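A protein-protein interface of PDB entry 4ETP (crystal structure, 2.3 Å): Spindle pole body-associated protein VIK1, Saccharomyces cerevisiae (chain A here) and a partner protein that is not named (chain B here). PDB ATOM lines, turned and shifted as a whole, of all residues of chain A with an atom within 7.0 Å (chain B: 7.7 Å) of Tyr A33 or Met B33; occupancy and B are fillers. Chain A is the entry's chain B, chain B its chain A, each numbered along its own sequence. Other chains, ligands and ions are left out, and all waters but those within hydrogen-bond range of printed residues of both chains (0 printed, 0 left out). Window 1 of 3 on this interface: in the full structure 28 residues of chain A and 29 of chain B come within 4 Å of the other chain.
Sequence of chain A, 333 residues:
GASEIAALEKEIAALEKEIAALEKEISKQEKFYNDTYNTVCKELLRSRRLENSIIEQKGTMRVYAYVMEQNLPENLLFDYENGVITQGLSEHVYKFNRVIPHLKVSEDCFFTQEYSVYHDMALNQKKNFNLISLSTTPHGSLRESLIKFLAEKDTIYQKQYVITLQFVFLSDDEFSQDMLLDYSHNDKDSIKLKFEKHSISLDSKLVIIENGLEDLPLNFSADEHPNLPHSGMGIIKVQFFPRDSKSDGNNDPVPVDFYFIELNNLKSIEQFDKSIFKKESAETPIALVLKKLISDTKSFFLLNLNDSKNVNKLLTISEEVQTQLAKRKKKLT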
ATOM      1  N   LYS A  28     -10.269  -8.268 -36.425  1.00  0.00           N
ATOM      2  CA  LYS A  28      -9.981  -9.674 -36.140  1.00  0.00           C
ATOM      3  C   LYS A  28      -9.453  -9.841 -34.715  1.00  0.00           C
ATOM      4  O   LYS A  28      -9.868 -10.747 -33.992  1.00  0.00           O
ATOM      5  CB  LYS A  28      -8.971 -10.223 -37.155  1.00  0.00           C
ATOM      6  CG  LYS A  28      -8.767 -11.730 -37.093  1.00  0.00           C
ATOM      7  CD  LYS A  28      -7.799 -12.200 -38.168  1.00  0.00           C
ATOM      8  CE  LYS A  28      -7.598 -13.705 -38.110  1.00  0.00           C
ATOM      9  NZ  LYS A  28      -6.646 -14.179 -39.152  1.00  0.00           N
ATOM     10  N   GLN A  29      -8.550  -8.946 -34.327  1.00  0.00           N
ATOM     11  CA  GLN A  29      -7.932  -8.943 -33.004  1.00  0.00           C
ATOM     12  C   GLN A  29      -8.962  -8.743 -31.888  1.00  0.00           C
ATOM     13  O   GLN A  29      -8.835  -9.323 -30.807  1.00  0.00           O
ATOM     14  CB  GLN A  29      -6.882  -7.835 -32.950  1.00  0.00           C
ATOM     15  CG  GLN A  29      -5.781  -8.028 -31.925  1.00  0.00           C
ATOM     16  CD  GLN A  29      -4.713  -6.951 -32.010  1.00  0.00           C
ATOM     17  OE1 GLN A  29      -3.608  -7.121 -31.496  1.00  0.00           O
ATOM     18  NE2 GLN A  29      -5.038  -5.835 -32.658  1.00  0.00           N
ATOM     19  N   GLU A  30      -9.979  -7.930 -32.167  1.00  0.00           N
ATOM     20  CA  GLU A  30     -11.046  -7.627 -31.212  1.00  0.00           C
ATOM     21  C   GLU A  30     -11.839  -8.879 -30.832  1.00  0.00           C
ATOM     22  O   GLU A  30     -12.206  -9.058 -29.666  1.00  0.00           O
ATOM     23  CB  GLU A  30     -11.976  -6.557 -31.792  1.00  0.00           C
ATOM     24  CG  GLU A  30     -13.036  -6.034 -30.829  1.00  0.00           C
ATOM     25  CD  GLU A  30     -14.046  -5.120 -31.504  1.00  0.00           C
ATOM     26  OE1 GLU A  30     -14.181  -5.174 -32.746  1.00  0.00           O
ATOM     27  OE2 GLU A  30     -14.712  -4.343 -30.790  1.00  0.00           O
ATOM     28  N   LYS A  31     -12.093  -9.733 -31.823  1.00  0.00           N
ATOM     29  CA  LYS A  31     -12.776 -11.009 -31.624  1.00  0.00           C
ATOM     30  C   LYS A  31     -12.021 -11.881 -30.619  1.00  0.00           C
ATOM     31  O   LYS A  31     -12.613 -12.369 -29.657  1.00  0.00           O
ATOM     32  CB  LYS A  31     -12.938 -11.743 -32.962  1.00  0.00           C
ATOM     33  CG  LYS A  31     -13.462 -13.169 -32.853  1.00  0.00           C
ATOM     34  CD  LYS A  31     -13.241 -13.935 -34.150  1.00  0.00           C
ATOM     35  CE  LYS A  31     -13.598 -15.408 -34.005  1.00  0.00           C
ATOM     36  NZ  LYS A  31     -15.062 -15.633 -33.852  1.00  0.00           N
ATOM     37  N   PHE A  32     -10.720 -12.066 -30.852  1.00  0.00           N
ATOM     38  CA  PHE A  32      -9.859 -12.829 -29.945  1.00  0.00           C
ATOM     39  C   PHE A  32      -9.807 -12.207 -28.553  1.00  0.00           C
ATOM     40  O   PHE A  32      -9.941 -12.913 -27.554  1.00  0.00           O
ATOM     41  CB  PHE A  32      -8.439 -12.959 -30.506  1.00  0.00           C
ATOM     42  CG  PHE A  32      -8.329 -13.888 -31.682  1.00  0.00           C
ATOM     43  CD1 PHE A  32      -8.540 -15.257 -31.530  1.00  0.00           C
ATOM     44  CD2 PHE A  32      -7.991 -13.399 -32.940  1.00  0.00           C
ATOM     45  CE1 PHE A  32      -8.431 -16.116 -32.614  1.00  0.00           C
ATOM     46  CE2 PHE A  32      -7.880 -14.254 -34.027  1.00  0.00           C
ATOM     47  CZ  PHE A  32      -8.101 -15.614 -33.864  1.00  0.00           C
ATOM     48  N   TYR A  33      -9.617 -10.887 -28.497  1.00  0.00           N
ATOM     49  CA  TYR A  33      -9.563 -10.158 -27.228  1.00  0.00           C
ATOM     50  C   TYR A  33     -10.844 -10.355 -26.408  1.00  0.00           C
ATOM     51  O   TYR A  33     -10.778 -10.640 -25.210  1.00  0.00           O
ATOM     52  CB  TYR A  33      -9.285  -8.658 -27.449  1.00  0.00           C
ATOM     53  CG  TYR A  33      -9.212  -7.879 -26.152  1.00  0.00           C
ATOM     54  CD1 TYR A  33      -7.995  -7.700 -25.491  1.00  0.00           C
ATOM     55  CD2 TYR A  33     -10.364  -7.347 -25.567  1.00  0.00           C
ATOM     56  CE1 TYR A  33      -7.926  -7.007 -24.291  1.00  0.00           C
ATOM     57  CE2 TYR A  33     -10.304  -6.654 -24.366  1.00  0.00           C
ATOM     58  CZ  TYR A  33      -9.084  -6.486 -23.735  1.00  0.00           C
ATOM     59  OH  TYR A  33      -9.017  -5.797 -22.546  1.00  0.00           O
ATOM     60  N   ASN A  34     -11.994 -10.203 -27.066  1.00  0.00           N
ATOM     61  CA  ASN A  34     -13.310 -10.398 -26.439  1.00  0.00           C
ATOM     62  C   ASN A  34     -13.515 -11.803 -25.872  1.00  0.00           C
ATOM     63  O   ASN A  34     -14.080 -11.957 -24.789  1.00  0.00           O
ATOM     64  CB  ASN A  34     -14.442 -10.071 -27.426  1.00  0.00           C
ATOM     65  CG  ASN A  34     -14.631  -8.577 -27.637  1.00  0.00           C
ATOM     66  OD1 ASN A  34     -14.124  -7.754 -26.872  1.00  0.00           O
ATOM     67  ND2 ASN A  34     -15.378  -8.219 -28.679  1.00  0.00           N
ATOM     68  N   ASP A  35     -13.069 -12.814 -26.617  1.00  0.00           N
ATOM     69  CA  ASP A  35     -13.137 -14.209 -26.174  1.00  0.00           C
ATOM     70  C   ASP A  35     -12.311 -14.426 -24.907  1.00  0.00           C
ATOM     71  O   ASP A  35     -12.785 -15.029 -23.948  1.00  0.00           O
ATOM     72  CB  ASP A  35     -12.646 -15.159 -27.278  1.00  0.00           C
ATOM     73  CG  ASP A  35     -13.588 -15.219 -28.475  1.00  0.00           C
ATOM     74  OD1 ASP A  35     -14.790 -14.903 -28.329  1.00  0.00           O
ATOM     75  OD2 ASP A  35     -13.118 -15.598 -29.570  1.00  0.00           O
ATOM     76  N   THR A  36     -11.078 -13.922 -24.916  1.00  0.00           N
ATOM     77  CA  THR A  36     -10.162 -14.058 -23.784  1.00  0.00           C
ATOM     78  C   THR A  36     -10.658 -13.264 -22.577  1.00  0.00           C
ATOM     79  O   THR A  36     -10.570 -13.735 -21.442  1.00  0.00           O
ATOM     80  CB  THR A  36      -8.736 -13.609 -24.163  1.00  0.00           C
ATOM     81  OG1 THR A  36      -8.397 -14.147 -25.447  1.00  0.00           O
ATOM     82  CG2 THR A  36      -7.721 -14.092 -23.133  1.00  0.00           C
ATOM     83  N   TYR A  37     -11.185 -12.069 -22.838  1.00  0.00           N
ATOM     84  CA  TYR A  37     -11.745 -11.206 -21.801  1.00  0.00           C
ATOM     85  C   TYR A  37     -12.937 -11.875 -21.113  1.00  0.00           C
ATOM     86  O   TYR A  37     -13.043 -11.850 -19.887  1.00  0.00           O
ATOM     87  CB  TYR A  37     -12.154  -9.858 -22.408  1.00  0.00           C
ATOM     88  CG  TYR A  37     -12.709  -8.845 -21.429  1.00  0.00           C
ATOM     89  CD1 TYR A  37     -11.869  -8.154 -20.555  1.00  0.00           C
ATOM     90  CD2 TYR A  37     -14.072  -8.558 -21.398  1.00  0.00           C
ATOM     91  CE1 TYR A  37     -12.375  -7.216 -19.665  1.00  0.00           C
ATOM     92  CE2 TYR A  37     -14.588  -7.622 -20.514  1.00  0.00           C
ATOM     93  CZ  TYR A  37     -13.737  -6.956 -19.649  1.00  0.00           C
ATOM     94  OH  TYR A  37     -14.250  -6.029 -18.770  1.00  0.00           O
ATOM     95  N   ASN A  38     -13.822 -12.473 -21.909  1.00  0.00           N
ATOM     96  CA  ASN A  38     -14.977 -13.197 -21.376  1.00  0.00           C
ATOM     97  C   ASN A  38     -14.581 -14.455 -20.604  1.00  0.00           C
ATOM     98  O   ASN A  38     -15.158 -14.746 -19.556  1.00  0.00           O
ATOM     99  CB  ASN A  38     -15.983 -13.526 -22.487  1.00  0.00           C
ATOM    100  CG  ASN A  38     -16.726 -12.296 -22.984  1.00  0.00           C
ATOM    101  OD1 ASN A  38     -16.976 -11.358 -22.225  1.00  0.00           O
ATOM    102  ND2 ASN A  38     -17.082 -12.295 -24.265  1.00  0.00           N
ATOM    103  N   THR A  39     -13.591 -15.186 -21.120  1.00  0.00           N
ATOM    104  CA  THR A  39     -13.053 -16.365 -20.430  1.00  0.00           C
ATOM    105  C   THR A  39     -12.492 -15.999 -19.047  1.00  0.00           C
ATOM    106  O   THR A  39     -12.793 -16.670 -18.061  1.00  0.00           O
ATOM    107  CB  THR A  39     -11.990 -17.094 -21.281  1.00  0.00           C
ATOM    108  OG1 THR A  39     -12.521 -17.347 -22.586  1.00  0.00           O
ATOM    109  CG2 THR A  39     -11.595 -18.428 -20.645  1.00  0.00           C
ATOM    110  N   LYS B  27      -0.578  -3.035 -30.938  1.00  0.00           N
ATOM    111  CA  LYS B  27       0.445  -3.351 -29.941  1.00  0.00           C
ATOM    112  C   LYS B  27      -0.127  -3.365 -28.522  1.00  0.00           C
ATOM    113  O   LYS B  27       0.262  -4.198 -27.702  1.00  0.00           O
ATOM    114  CB  LYS B  27       1.612  -2.363 -30.035  1.00  0.00           C
ATOM    115  CG  LYS B  27       2.894  -2.842 -29.374  1.00  0.00           C
ATOM    116  CD  LYS B  27       3.984  -1.782 -29.446  1.00  0.00           C
ATOM    117  CE  LYS B  27       5.245  -2.245 -28.736  1.00  0.00           C
ATOM    118  NZ  LYS B  27       6.319  -1.214 -28.779  1.00  0.00           N
ATOM    119  N   ASP B  28      -1.050  -2.445 -28.244  1.00  0.00           N
ATOM    120  CA  ASP B  28      -1.689  -2.357 -26.931  1.00  0.00           C
ATOM    121  C   ASP B  28      -2.603  -3.554 -26.679  1.00  0.00           C
ATOM    122  O   ASP B  28      -2.607  -4.122 -25.584  1.00  0.00           O
ATOM    123  CB  ASP B  28      -2.477  -1.049 -26.793  1.00  0.00           C
ATOM    124  CG  ASP B  28      -2.729  -0.668 -25.341  1.00  0.00           C
ATOM    125  OD1 ASP B  28      -1.748  -0.418 -24.607  1.00  0.00           O
ATOM    126  OD2 ASP B  28      -3.910  -0.609 -24.935  1.00  0.00           O
ATOM    127  N   THR B  29      -3.365  -3.932 -27.703  1.00  0.00           N
ATOM    128  CA  THR B  29      -4.278  -5.071 -27.634  1.00  0.00           C
ATOM    129  C   THR B  29      -3.514  -6.388 -27.440  1.00  0.00           C
ATOM    130  O   THR B  29      -3.949  -7.248 -26.673  1.00  0.00           O
ATOM    131  CB  THR B  29      -5.182  -5.132 -28.882  1.00  0.00           C
ATOM    132  OG1 THR B  29      -5.757  -3.842 -29.110  1.00  0.00           O
ATOM    133  CG2 THR B  29      -6.305  -6.143 -28.701  1.00  0.00           C
ATOM    134  N   GLU B  30      -2.374  -6.527 -28.121  1.00  0.00           N
ATOM    135  CA  GLU B  30      -1.478  -7.674 -27.937  1.00  0.00           C
ATOM    136  C   GLU B  30      -0.996  -7.764 -26.490  1.00  0.00           C
ATOM    137  O   GLU B  30      -0.968  -8.848 -25.906  1.00  0.00           O
ATOM    138  CB  GLU B  30      -0.269  -7.587 -28.875  1.00  0.00           C
ATOM    139  CG  GLU B  30      -0.559  -7.940 -30.325  1.00  0.00           C
ATOM    140  CD  GLU B  30       0.603  -7.644 -31.261  1.00  0.00           C
ATOM    141  OE1 GLU B  30       1.563  -6.954 -30.846  1.00  0.00           O
ATOM    142  OE2 GLU B  30       0.555  -8.100 -32.424  1.00  0.00           O
ATOM    143  N   LEU B  31      -0.624  -6.615 -25.930  1.00  0.00           N
ATOM    144  CA  LEU B  31      -0.178  -6.515 -24.544  1.00  0.00           C
ATOM    145  C   LEU B  31      -1.303  -6.863 -23.566  1.00  0.00           C
ATOM    146  O   LEU B  31      -1.083  -7.589 -22.593  1.00  0.00           O
ATOM    147  CB  LEU B  31       0.361  -5.107 -24.265  1.00  0.00           C
ATOM    148  CG  LEU B  31       1.126  -4.828 -22.969  1.00  0.00           C
ATOM    149  CD1 LEU B  31       2.539  -5.397 -23.022  1.00  0.00           C
ATOM    150  CD2 LEU B  31       1.167  -3.330 -22.700  1.00  0.00           C
ATOM    151  N   GLY B  32      -2.501  -6.344 -23.833  1.00  0.00           N
ATOM    152  CA  GLY B  32      -3.684  -6.634 -23.026  1.00  0.00           C
ATOM    153  C   GLY B  32      -4.036  -8.113 -23.011  1.00  0.00           C
ATOM    154  O   GLY B  32      -4.306  -8.677 -21.949  1.00  0.00           O
ATOM    155  N   MET B  33      -4.024  -8.732 -24.191  1.00  0.00           N
ATOM    156  CA  MET B  33      -4.276 -10.167 -24.332  1.00  0.00           C
ATOM    157  C   MET B  33      -3.234 -11.012 -23.608  1.00  0.00           C
ATOM    158  O   MET B  33      -3.578 -11.987 -22.935  1.00  0.00           O
ATOM    159  CB  MET B  33      -4.359 -10.568 -25.806  1.00  0.00           C
ATOM    160  CG  MET B  33      -5.772 -10.520 -26.362  1.00  0.00           C
ATOM    161  SD  MET B  33      -6.026 -11.608 -27.776  1.00  0.00           S
ATOM    162  CE  MET B  33      -5.783 -13.220 -27.034  1.00  0.00           C
ATOM    163  N   LYS B  34      -1.969 -10.619 -23.746  1.00  0.00           N
ATOM    164  CA  LYS B  34      -0.862 -11.237 -23.021  1.00  0.00           C
ATOM    165  C   LYS B  34      -1.131 -11.220 -21.515  1.00  0.00           C
ATOM    166  O   LYS B  34      -0.939 -12.230 -20.833  1.00  0.00           O
ATOM    167  CB  LYS B  34       0.450 -10.512 -23.349  1.00  0.00           C
ATOM    168  CG  LYS B  34       1.698 -11.111 -22.718  1.00  0.00           C
ATOM    169  CD  LYS B  34       2.916 -10.233 -22.980  1.00  0.00           C
ATOM    170  CE  LYS B  34       4.160 -10.762 -22.278  1.00  0.00           C
ATOM    171  NZ  LYS B  34       4.661 -12.020 -22.894  1.00  0.00           N
ATOM    172  N   GLU B  35      -1.588 -10.073 -21.015  1.00  0.00           N
ATOM    173  CA  GLU B  35      -1.925  -9.904 -19.599  1.00  0.00           C
ATOM    174  C   GLU B  35      -3.148 -10.726 -19.187  1.00  0.00           C
ATOM    175  O   GLU B  35      -3.159 -11.313 -18.105  1.00  0.00           O
ATOM    176  CB  GLU B  35      -2.143  -8.424 -19.267  1.00  0.00           C
ATOM    177  CG  GLU B  35      -0.862  -7.602 -19.233  1.00  0.00           C
ATOM    178  CD  GLU B  35      -1.105  -6.102 -19.299  1.00  0.00           C
ATOM    179  OE1 GLU B  35      -0.153  -5.340 -19.024  1.00  0.00           O
ATOM    180  OE2 GLU B  35      -2.237  -5.680 -19.627  1.00  0.00           O
ATOM    181  N   LEU B  36      -4.169 -10.767 -20.046  1.00  0.00           N
ATOM    182  CA  LEU B  36      -5.354 -11.589 -19.784  1.00  0.00           C
ATOM    183  C   LEU B  36      -5.000 -13.076 -19.720  1.00  0.00           C
ATOM    184  O   LEU B  36      -5.520 -13.806 -18.880  1.00  0.00           O
ATOM    185  CB  LEU B  36      -6.437 -11.354 -20.838  1.00  0.00           C
ATOM    186  CG  LEU B  36      -7.210 -10.034 -20.840  1.00  0.00           C
ATOM    187  CD1 LEU B  36      -8.092  -9.973 -22.076  1.00  0.00           C
ATOM    188  CD2 LEU B  36      -8.046  -9.858 -19.578  1.00  0.00           C
ATOM    189  N   ASN B  37      -4.106 -13.507 -20.609  1.00  0.00           N
ATOM    190  CA  ASN B  37      -3.659 -14.894 -20.657  1.00  0.00           C
ATOM    191  C   ASN B  37      -2.817 -15.307 -19.451  1.00  0.00           C
ATOM    192  O   ASN B  37      -2.869 -16.463 -19.029  1.00  0.00           O
ATOM    193  CB  ASN B  37      -2.922 -15.183 -21.968  1.00  0.00           C
ATOM    194  CG  ASN B  37      -3.870 -15.533 -23.102  1.00  0.00           C
ATOM    195  OD1 ASN B  37      -4.679 -16.457 -22.991  1.00  0.00           O
ATOM    196  ND2 ASN B  37      -3.772 -14.798 -24.206  1.00  0.00           N
ATOM    197  N   GLU B  38      -2.060 -14.365 -18.893  1.00  0.00           N
ATOM    198  CA  GLU B  38      -1.295 -14.621 -17.670  1.00  0.00           C
ATOM    199  C   GLU B  38      -2.218 -14.764 -16.462  1.00  0.00           C
ATOM    200  O   GLU B  38      -1.937 -15.540 -15.550  1.00  0.00           O
ATOM    201  CB  GLU B  38      -0.233 -13.541 -17.433  1.00  0.00           C
ATOM    202  CG  GLU B  38       0.960 -13.644 -18.377  1.00  0.00           C
ATOM    203  CD  GLU B  38       2.173 -12.845 -17.924  1.00  0.00           C
ATOM    204  OE1 GLU B  38       2.106 -12.159 -16.881  1.00  0.00           O
ATOM    205  OE2 GLU B  38       3.208 -12.909 -18.620  1.00  0.00           O
ATOM    206  N   ILE B  39      -3.319 -14.016 -16.467  1.00  0.00           N
ATOM    207  CA  ILE B  39      -4.363 -14.162 -15.451  1.00  0.00           C
ATOM    208  C   ILE B  39      -4.996 -15.556 -15.544  1.00  0.00           C
ATOM    209  O   ILE B  39      -5.158 -16.230 -14.530  1.00  0.00           O
ATOM    210  CB  ILE B  39      -5.432 -13.050 -15.572  1.00  0.00           C
ATOM    211  CG1 ILE B  39      -4.831 -11.700 -15.158  1.00  0.00           C
ATOM    212  CG2 ILE B  39      -6.660 -13.374 -14.725  1.00  0.00           C
ATOM    213  CD1 ILE B  39      -5.623 -10.496 -15.628  1.00  0.00           C
ATOM    214  N   LEU B  40      -5.321 -15.985 -16.764  1.00  0.00           N
ATOM    215  CA  LEU B  40      -5.871 -17.323 -17.002  1.00  0.00           C
ATOM    216  C   LEU B  40      -4.934 -18.426 -16.525  1.00  0.00           C
ATOM    217  O   LEU B  40      -5.367 -19.355 -15.845  1.00  0.00           O
ATOM    218  CB  LEU B  40      -6.212 -17.532 -18.485  1.00  0.00           C
ATOM    219  CG  LEU B  40      -7.444 -16.807 -19.036  1.00  0.00           C
ATOM    220  CD1 LEU B  40      -7.543 -16.972 -20.548  1.00  0.00           C
ATOM    221  CD2 LEU B  40      -8.716 -17.290 -18.347  1.00  0.00           C
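Of the printed residues of chain B, Tyr A33 touches Thr B29 (3.9 Å), Met B33 (3.7 Å) and Leu B36 (3.7 Å). Printed residues of chain B within 4 Å of Thr A39: Leu B40. Of the printed residues of chain A, Thr B29 touches Gln A29 and Tyr A33. Leu B31 touches none of the printed residues of chain A. Of chain A, only Phe A32 (3.9 Å), Tyr A33 (3.7 Å) and Thr A36 (3.2 Å) come within 4 Å of Met B33. Ile B39 touches none of the printed residues of chain A. The nearest residue of chain B that does not touch Tyr A33 is Gly B32 (4.2 Å). The nearest residue of chain A that does not touch Met B33 is Gln A29 (4.7 Å). The nearest printed residue of chain B that does not touch Gln A29 is Met B33 (4.7 Å).
Of the 12 printed residues of chain A, 6 touch a printed residue of chain B. Of the 14 printed residues of chain B, 6 touch a printed residue of chain A. Hydrophobic or aromatic side chains of chain B that line the printed part of chain A: Met B33, Leu B36 and Leu B40. Among the printed residues, no Asp or Glu carboxylate lies within 4 Å of a Lys or Arg side-chain nitrogen of the other chain.
ND2 of Asn B37 lies within hydrogen-bond range of O of Met B33 (3.1 Å). The backbone carbonyl oxygen (O) of Phe A32 sits at hydrogen-bond distance from the side-chain hydroxyl (OG1) of Thr A36, at 2.9 Å. O of Asp A35 lies within hydrogen-bond range of OG1 of Thr A39, at 2.7 Å.
Among the printed residues, merely in contact across the chains: Thr A36 with Met B33 (3.2 Å), Gln A29 with Glu B30 (3.4 Å), Gln A29 with Thr B29 (3.6 Å), Tyr A33 with Leu B36 (3.7 Å), Thr A36 with Leu B36 (3.8 Å), Tyr A37 with Leu B36 (3.8 Å), Thr A39 with Leu B40 (3.9 Å), Thr A36 with Asn B37 (3.9 Å), Thr A36 with Leu B40 (3.9 Å), Phe A32 with Met B33 (3.9 Å) and Tyr A33 with Thr B29 (3.9 Å).
SD of Met B33 lies within hydrogen-bond range of N of Tyr A33, at 3.7 Å.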
